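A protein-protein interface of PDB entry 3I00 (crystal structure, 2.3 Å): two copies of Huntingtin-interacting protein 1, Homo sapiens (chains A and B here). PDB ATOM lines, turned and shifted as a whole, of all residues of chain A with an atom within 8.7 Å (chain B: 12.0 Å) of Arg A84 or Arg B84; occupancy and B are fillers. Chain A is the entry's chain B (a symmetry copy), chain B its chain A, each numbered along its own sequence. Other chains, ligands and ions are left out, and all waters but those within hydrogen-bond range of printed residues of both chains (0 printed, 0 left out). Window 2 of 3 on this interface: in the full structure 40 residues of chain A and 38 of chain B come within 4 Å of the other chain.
The side-chain carboxylate (OE1) of Glu B76 lies within salt-bridge range of the guanidinium group (NH1) of Arg A81 (3.0 Å).
The guanidinium group (NH1) of Arg A84 lies within hydrogen-bond range of the backbone carbonyl oxygen (O) of Leu B80 (2.8 Å).
Arg A84 touches just these residues of chain B: Leu B80, Arg B81 and Arg B84.
Arg B84 touches just one residue of chain A: Arg A84.
No residue of chain B comes within 4 Å of Arg A82.
No residue of chain B comes within 4 Å of Gln A83.
No residue of chain B comes within 4 Å of Asp A86.
Of the printed residues of chain B, Leu A77 touches Glu B76 (3.99 Å).
Of the printed residues of chain B, Arg A81 touches Glu B76 and Leu B80.
Gln B83 touches none of the printed residues of chain A.
The nearest printed residue of chain A that does not touch Arg B81 is Leu A77 (6.3 Å).
Leu B80 touches its own counterpart, Leu A80.
Arg A84 touches Leu B80, but with the chains exchanged Leu A80 does not touch Arg B84 (7.3 Å).
Arg A84 touches Arg B81, but with the chains exchanged Arg A81 does not touch Arg B84 (7.7 Å).
Arg A84 touches its own counterpart, Arg B84.
9 positions are printed for both chains.
Of the 8 pairs that touch across the chains among the printed residues, 4 have their exchanged pair printed and touching as well.
Among the printed residues, pairs that only touch across the chains: Leu A77 with Glu B76 (3.99 Å), Leu A80 with Leu B80 (3.6 Å), Leu A80 with Arg B81 (3.97 Å), Arg A81 with Leu B80 (3.6 Å), Arg A84 with Arg B81 (3.4 Å) and Arg A84 with Arg B84 (3.4 Å).
Among the printed residues, 8 pairs touch across the chains.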
ATOM      1  N   LEU A  77       0.767 -15.427 -24.397  1.00  0.00           N
ATOM      2  CA  LEU A  77       0.475 -15.925 -23.042  1.00  0.00           C
ATOM      3  C   LEU A  77      -0.004 -17.377 -22.994  1.00  0.00           C
ATOM      4  O   LEU A  77       0.599 -18.198 -22.313  1.00  0.00           O
ATOM      5  CB  LEU A  77      -0.564 -15.029 -22.355  1.00  0.00           C
ATOM      6  CG  LEU A  77      -0.077 -13.854 -21.502  1.00  0.00           C
ATOM      7  CD1 LEU A  77      -1.169 -12.765 -21.348  1.00  0.00           C
ATOM      8  CD2 LEU A  77       0.397 -14.324 -20.139  1.00  0.00           C
ATOM      9  N   ASP A  78      -1.095 -17.670 -23.706  1.00  0.00           N
ATOM     10  CA  ASP A  78      -1.699 -19.007 -23.762  1.00  0.00           C
ATOM     11  C   ASP A  78      -0.697 -20.102 -24.172  1.00  0.00           C
ATOM     12  O   ASP A  78      -0.597 -21.150 -23.528  1.00  0.00           O
ATOM     13  CB  ASP A  78      -2.892 -19.012 -24.729  1.00  0.00           C
ATOM     14  CG  ASP A  78      -4.098 -18.258 -24.192  1.00  0.00           C
ATOM     15  OD1 ASP A  78      -3.934 -17.482 -23.227  1.00  0.00           O
ATOM     16  OD2 ASP A  78      -5.211 -18.425 -24.747  1.00  0.00           O
ATOM     17  N   GLU A  79       0.045 -19.831 -25.241  1.00  0.00           N
ATOM     18  CA  GLU A  79       1.017 -20.778 -25.761  1.00  0.00           C
ATOM     19  C   GLU A  79       2.258 -20.964 -24.903  1.00  0.00           C
ATOM     20  O   GLU A  79       2.726 -22.081 -24.736  1.00  0.00           O
ATOM     21  CB  GLU A  79       1.423 -20.444 -27.197  1.00  0.00           C
ATOM     22  CG  GLU A  79       2.340 -21.494 -27.813  1.00  0.00           C
ATOM     23  CD  GLU A  79       1.655 -22.838 -28.031  1.00  0.00           C
ATOM     24  OE1 GLU A  79       2.384 -23.815 -28.274  1.00  0.00           O
ATOM     25  OE2 GLU A  79       0.402 -22.924 -27.988  1.00  0.00           O
ATOM     26  N   LEU A  80       2.809 -19.885 -24.369  1.00  0.00           N
ATOM     27  CA  LEU A  80       4.015 -20.022 -23.565  1.00  0.00           C
ATOM     28  C   LEU A  80       3.756 -20.904 -22.341  1.00  0.00           C
ATOM     29  O   LEU A  80       4.627 -21.706 -21.973  1.00  0.00           O
ATOM     30  CB  LEU A  80       4.615 -18.665 -23.197  1.00  0.00           C
ATOM     31  CG  LEU A  80       5.947 -18.665 -22.411  1.00  0.00           C
ATOM     32  CD1 LEU A  80       7.048 -19.530 -23.056  1.00  0.00           C
ATOM     33  CD2 LEU A  80       6.434 -17.239 -22.185  1.00  0.00           C
ATOM     34  N   ARG A  81       2.555 -20.781 -21.751  1.00  0.00           N
ATOM     35  CA  ARG A  81       2.092 -21.680 -20.667  1.00  0.00           C
ATOM     36  C   ARG A  81       1.877 -23.108 -21.153  1.00  0.00           C
ATOM     37  O   ARG A  81       2.176 -24.064 -20.439  1.00  0.00           O
ATOM     38  CB  ARG A  81       0.786 -21.188 -20.046  1.00  0.00           C
ATOM     39  CG  ARG A  81       0.762 -19.717 -19.670  1.00  0.00           C
ATOM     40  CD  ARG A  81      -0.147 -19.501 -18.460  1.00  0.00           C
ATOM     41  NE  ARG A  81      -1.039 -18.352 -18.584  1.00  0.00           N
ATOM     42  CZ  ARG A  81      -0.853 -17.173 -17.990  1.00  0.00           C
ATOM     43  NH1 ARG A  81      -1.754 -16.211 -18.152  1.00  0.00           N
ATOM     44  NH2 ARG A  81       0.214 -16.952 -17.224  1.00  0.00           N
ATOM     45  N   ARG A  82       1.340 -23.241 -22.366  1.00  0.00           N
ATOM     46  CA  ARG A  82       1.037 -24.544 -22.966  1.00  0.00           C
ATOM     47  C   ARG A  82       2.334 -25.339 -23.122  1.00  0.00           C
ATOM     48  O   ARG A  82       2.411 -26.525 -22.784  1.00  0.00           O
ATOM     49  CB  ARG A  82       0.396 -24.334 -24.343  1.00  0.00           C
ATOM     50  CG  ARG A  82      -0.856 -25.119 -24.592  1.00  0.00           C
ATOM     51  CD  ARG A  82      -1.004 -25.458 -26.072  1.00  0.00           C
ATOM     52  NE  ARG A  82      -0.497 -26.800 -26.353  1.00  0.00           N
ATOM     53  CZ  ARG A  82       0.664 -27.078 -26.946  1.00  0.00           C
ATOM     54  NH1 ARG A  82       1.463 -26.103 -27.360  1.00  0.00           N
ATOM     55  NH2 ARG A  82       1.022 -28.346 -27.133  1.00  0.00           N
ATOM     56  N   GLN A  83       3.343 -24.647 -23.642  1.00  0.00           N
ATOM     57  CA  GLN A  83       4.660 -25.193 -23.914  1.00  0.00           C
ATOM     58  C   GLN A  83       5.363 -25.578 -22.617  1.00  0.00           C
ATOM     59  O   GLN A  83       6.136 -26.539 -22.585  1.00  0.00           O
ATOM     60  CB  GLN A  83       5.488 -24.142 -24.653  1.00  0.00           C
ATOM     61  CG  GLN A  83       5.025 -23.846 -26.079  1.00  0.00           C
ATOM     62  CD  GLN A  83       5.475 -24.908 -27.055  1.00  0.00           C
ATOM     63  OE1 GLN A  83       6.653 -25.234 -27.115  1.00  0.00           O
ATOM     64  NE2 GLN A  83       4.540 -25.462 -27.816  1.00  0.00           N
ATOM     65  N   ARG A  84       5.088 -24.824 -21.555  1.00  0.00           N
ATOM     66  CA  ARG A  84       5.658 -25.098 -20.240  1.00  0.00           C
ATOM     67  C   ARG A  84       4.992 -26.232 -19.452  1.00  0.00           C
ATOM     68  O   ARG A  84       5.676 -26.883 -18.655  1.00  0.00           O
ATOM     69  CB  ARG A  84       5.668 -23.837 -19.383  1.00  0.00           C
ATOM     70  CG  ARG A  84       6.732 -22.831 -19.754  1.00  0.00           C
ATOM     71  CD  ARG A  84       6.701 -21.681 -18.763  1.00  0.00           C
ATOM     72  NE  ARG A  84       7.620 -20.615 -19.126  1.00  0.00           N
ATOM     73  CZ  ARG A  84       7.718 -19.459 -18.483  1.00  0.00           C
ATOM     74  NH1 ARG A  84       6.956 -19.212 -17.424  1.00  0.00           N
ATOM     75  NH2 ARG A  84       8.592 -18.550 -18.892  1.00  0.00           N
ATOM     76  N   GLU A  85       3.688 -26.461 -19.641  1.00  0.00           N
ATOM     77  CA  GLU A  85       2.979 -27.561 -18.946  1.00  0.00           C
ATOM     78  C   GLU A  85       3.478 -28.961 -19.341  1.00  0.00           C
ATOM     79  O   GLU A  85       3.086 -29.971 -18.733  1.00  0.00           O
ATOM     80  CB  GLU A  85       1.465 -27.470 -19.140  1.00  0.00           C
ATOM     81  CG  GLU A  85       0.823 -26.256 -18.469  1.00  0.00           C
ATOM     82  CD  GLU A  85      -0.557 -25.941 -19.009  1.00  0.00           C
ATOM     83  OE1 GLU A  85      -1.355 -26.894 -19.134  1.00  0.00           O
ATOM     84  OE2 GLU A  85      -0.842 -24.748 -19.301  1.00  0.00           O
ATOM     85  N   ASP A  86       4.343 -29.020 -20.354  1.00  0.00           N
ATOM     86  CA  ASP A  86       5.047 -30.259 -20.688  1.00  0.00           C
ATOM     87  C   ASP A  86       6.378 -30.236 -19.941  1.00  0.00           C
ATOM     88  O   ASP A  86       6.513 -30.859 -18.888  1.00  0.00           O
ATOM     89  CB  ASP A  86       5.291 -30.391 -22.200  1.00  0.00           C
ATOM     90  CG  ASP A  86       4.238 -29.663 -23.040  1.00  0.00           C
ATOM     91  OD1 ASP A  86       3.094 -30.170 -23.147  1.00  0.00           O
ATOM     92  OD2 ASP A  86       4.565 -28.601 -23.609  1.00  0.00           O
ATOM     93  N   ARG B  74       0.565  -7.055 -21.666  1.00  0.00           N
ATOM     94  CA  ARG B  74       1.991  -6.956 -21.961  1.00  0.00           C
ATOM     95  C   ARG B  74       2.787  -7.189 -20.675  1.00  0.00           C
ATOM     96  O   ARG B  74       3.714  -7.994 -20.658  1.00  0.00           O
ATOM     97  CB  ARG B  74       2.304  -5.584 -22.566  1.00  0.00           C
ATOM     98  CG  ARG B  74       3.502  -5.510 -23.494  1.00  0.00           C
ATOM     99  CD  ARG B  74       3.534  -4.141 -24.213  1.00  0.00           C
ATOM    100  NE  ARG B  74       2.343  -3.914 -25.045  1.00  0.00           N
ATOM    101  CZ  ARG B  74       1.494  -2.886 -24.943  1.00  0.00           C
ATOM    102  NH1 ARG B  74       1.686  -1.898 -24.068  1.00  0.00           N
ATOM    103  NH2 ARG B  74       0.440  -2.833 -25.749  1.00  0.00           N
ATOM    104  N   ALA B  75       2.394  -6.514 -19.593  1.00  0.00           N
ATOM    105  CA  ALA B  75       3.033  -6.700 -18.281  1.00  0.00           C
ATOM    106  C   ALA B  75       2.879  -8.129 -17.731  1.00  0.00           C
ATOM    107  O   ALA B  75       3.840  -8.697 -17.214  1.00  0.00           O
ATOM    108  CB  ALA B  75       2.522  -5.667 -17.276  1.00  0.00           C
ATOM    109  N   GLU B  76       1.678  -8.699 -17.861  1.00  0.00           N
ATOM    110  CA  GLU B  76       1.409 -10.090 -17.483  1.00  0.00           C
ATOM    111  C   GLU B  76       2.290 -11.102 -18.261  1.00  0.00           C
ATOM    112  O   GLU B  76       2.698 -12.125 -17.729  1.00  0.00           O
ATOM    113  CB  GLU B  76      -0.089 -10.414 -17.666  1.00  0.00           C
ATOM    114  CG  GLU B  76      -0.501 -11.801 -17.112  1.00  0.00           C
ATOM    115  CD  GLU B  76      -1.958 -12.187 -17.362  1.00  0.00           C
ATOM    116  OE1 GLU B  76      -2.244 -13.404 -17.295  1.00  0.00           O
ATOM    117  OE2 GLU B  76      -2.812 -11.305 -17.619  1.00  0.00           O
ATOM    118  N   LEU B  77       2.572 -10.804 -19.521  1.00  0.00           N
ATOM    119  CA  LEU B  77       3.437 -11.647 -20.344  1.00  0.00           C
ATOM    120  C   LEU B  77       4.904 -11.546 -19.916  1.00  0.00           C
ATOM    121  O   LEU B  77       5.609 -12.560 -19.891  1.00  0.00           O
ATOM    122  CB  LEU B  77       3.278 -11.327 -21.852  1.00  0.00           C
ATOM    123  CG  LEU B  77       4.138 -12.077 -22.905  1.00  0.00           C
ATOM    124  CD1 LEU B  77       4.049 -13.623 -22.823  1.00  0.00           C
ATOM    125  CD2 LEU B  77       3.832 -11.598 -24.312  1.00  0.00           C
ATOM    126  N   ASP B  78       5.358 -10.335 -19.599  1.00  0.00           N
ATOM    127  CA  ASP B  78       6.733 -10.109 -19.150  1.00  0.00           C
ATOM    128  C   ASP B  78       6.975 -10.823 -17.840  1.00  0.00           C
ATOM    129  O   ASP B  78       8.032 -11.416 -17.631  1.00  0.00           O
ATOM    130  CB  ASP B  78       7.019  -8.625 -18.943  1.00  0.00           C
ATOM    131  CG  ASP B  78       6.936  -7.816 -20.218  1.00  0.00           C
ATOM    132  OD1 ASP B  78       7.247  -8.338 -21.308  1.00  0.00           O
ATOM    133  OD2 ASP B  78       6.572  -6.628 -20.112  1.00  0.00           O
ATOM    134  N   GLU B  79       5.982 -10.737 -16.960  1.00  0.00           N
ATOM    135  CA  GLU B  79       6.004 -11.403 -15.667  1.00  0.00           C
ATOM    136  C   GLU B  79       6.122 -12.916 -15.842  1.00  0.00           C
ATOM    137  O   GLU B  79       7.011 -13.527 -15.256  1.00  0.00           O
ATOM    138  CB  GLU B  79       4.752 -11.036 -14.862  1.00  0.00           C
ATOM    139  CG  GLU B  79       4.601 -11.803 -13.547  1.00  0.00           C
ATOM    140  CD  GLU B  79       5.592 -11.368 -12.480  1.00  0.00           C
ATOM    141  OE1 GLU B  79       5.986 -10.181 -12.482  1.00  0.00           O
ATOM    142  OE2 GLU B  79       5.968 -12.220 -11.637  1.00  0.00           O
ATOM    143  N   LEU B  80       5.252 -13.503 -16.664  1.00  0.00           N
ATOM    144  CA  LEU B  80       5.289 -14.939 -16.952  1.00  0.00           C
ATOM    145  C   LEU B  80       6.653 -15.406 -17.479  1.00  0.00           C
ATOM    146  O   LEU B  80       7.194 -16.414 -17.001  1.00  0.00           O
ATOM    147  CB  LEU B  80       4.168 -15.315 -17.945  1.00  0.00           C
ATOM    148  CG  LEU B  80       3.610 -16.733 -18.240  1.00  0.00           C
ATOM    149  CD1 LEU B  80       3.830 -17.204 -19.691  1.00  0.00           C
ATOM    150  CD2 LEU B  80       4.001 -17.831 -17.245  1.00  0.00           C
ATOM    151  N   ARG B  81       7.204 -14.690 -18.461  1.00  0.00           N
ATOM    152  CA  ARG B  81       8.457 -15.123 -19.081  1.00  0.00           C
ATOM    153  C   ARG B  81       9.634 -14.954 -18.133  1.00  0.00           C
ATOM    154  O   ARG B  81      10.614 -15.694 -18.225  1.00  0.00           O
ATOM    155  CB  ARG B  81       8.695 -14.475 -20.455  1.00  0.00           C
ATOM    156  CG  ARG B  81       8.490 -12.978 -20.539  1.00  0.00           C
ATOM    157  CD  ARG B  81       8.390 -12.481 -22.001  1.00  0.00           C
ATOM    158  NE  ARG B  81       7.849 -13.499 -22.902  1.00  0.00           N
ATOM    159  CZ  ARG B  81       7.422 -13.289 -24.152  1.00  0.00           C
ATOM    160  NH1 ARG B  81       7.431 -12.066 -24.697  1.00  0.00           N
ATOM    161  NH2 ARG B  81       6.973 -14.327 -24.871  1.00  0.00           N
ATOM    162  N   ARG B  82       9.504 -14.006 -17.196  1.00  0.00           N
ATOM    163  CA  ARG B  82      10.504 -13.783 -16.135  1.00  0.00           C
ATOM    164  C   ARG B  82      10.436 -14.830 -15.027  1.00  0.00           C
ATOM    165  O   ARG B  82      11.264 -14.843 -14.133  1.00  0.00           O
ATOM    166  CB  ARG B  82      10.388 -12.371 -15.549  1.00  0.00           C
ATOM    167  CG  ARG B  82      11.031 -11.316 -16.432  1.00  0.00           C
ATOM    168  CD  ARG B  82      10.502  -9.927 -16.170  1.00  0.00           C
ATOM    169  NE  ARG B  82      10.966  -8.993 -17.196  1.00  0.00           N
ATOM    170  CZ  ARG B  82      10.421  -7.802 -17.453  1.00  0.00           C
ATOM    171  NH1 ARG B  82       9.371  -7.368 -16.764  1.00  0.00           N
ATOM    172  NH2 ARG B  82      10.932  -7.037 -18.413  1.00  0.00           N
ATOM    173  N   GLN B  83       9.464 -15.730 -15.103  1.00  0.00           N
ATOM    174  CA  GLN B  83       9.367 -16.808 -14.128  1.00  0.00           C
ATOM    175  C   GLN B  83      10.201 -18.029 -14.532  1.00  0.00           C
ATOM    176  O   GLN B  83      10.105 -19.104 -13.921  1.00  0.00           O
ATOM    177  CB  GLN B  83       7.900 -17.142 -13.851  1.00  0.00           C
ATOM    178  CG  GLN B  83       7.214 -15.968 -13.151  1.00  0.00           C
ATOM    179  CD  GLN B  83       5.750 -16.217 -12.841  1.00  0.00           C
ATOM    180  OE1 GLN B  83       5.032 -16.876 -13.613  1.00  0.00           O
ATOM    181  NE2 GLN B  83       5.291 -15.682 -11.694  1.00  0.00           N
ATOM    182  N   ARG B  84      11.032 -17.830 -15.557  1.00  0.00           N
ATOM    183  CA  ARG B  84      11.935 -18.851 -16.072  1.00  0.00           C
ATOM    184  C   ARG B  84      13.139 -18.199 -16.752  1.00  0.00           C
ATOM    185  O   ARG B  84      13.859 -18.861 -17.513  1.00  0.00           O
ATOM    186  CB  ARG B  84      11.215 -19.750 -17.081  1.00  0.00           C
ATOM    187  CG  ARG B  84      10.272 -20.776 -16.493  1.00  0.00           C
ATOM    188  CD  ARG B  84      11.017 -21.993 -15.950  1.00  0.00           C
ATOM    189  NE  ARG B  84      10.518 -23.244 -16.533  1.00  0.00           N
ATOM    190  CZ  ARG B  84       9.307 -23.771 -16.321  1.00  0.00           C
ATOM    191  NH1 ARG B  84       8.422 -23.160 -15.538  1.00  0.00           N
ATOM    192  NH2 ARG B  84       8.978 -24.911 -16.912  1.00  0.00           N
ATOM    193  N   GLU B  85      13.356 -16.917 -16.470  1.00  0.00           N
ATOM    194  CA  GLU B  85      14.355 -16.109 -17.170  1.00  0.00           C
ATOM    195  C   GLU B  85      15.804 -16.482 -16.819  1.00  0.00           C
ATOM    196  O   GLU B  85      16.068 -17.454 -16.103  1.00  0.00           O
ATOM    197  CB  GLU B  85      14.096 -14.621 -16.905  1.00  0.00           C
ATOM    198  CG  GLU B  85      14.915 -13.651 -17.757  1.00  0.00           C
ATOM    199  CD  GLU B  85      14.303 -13.359 -19.127  1.00  0.00           C
ATOM    200  OE1 GLU B  85      13.058 -13.456 -19.281  1.00  0.00           O
ATOM    201  OE2 GLU B  85      15.083 -13.013 -20.049  1.00  0.00           O
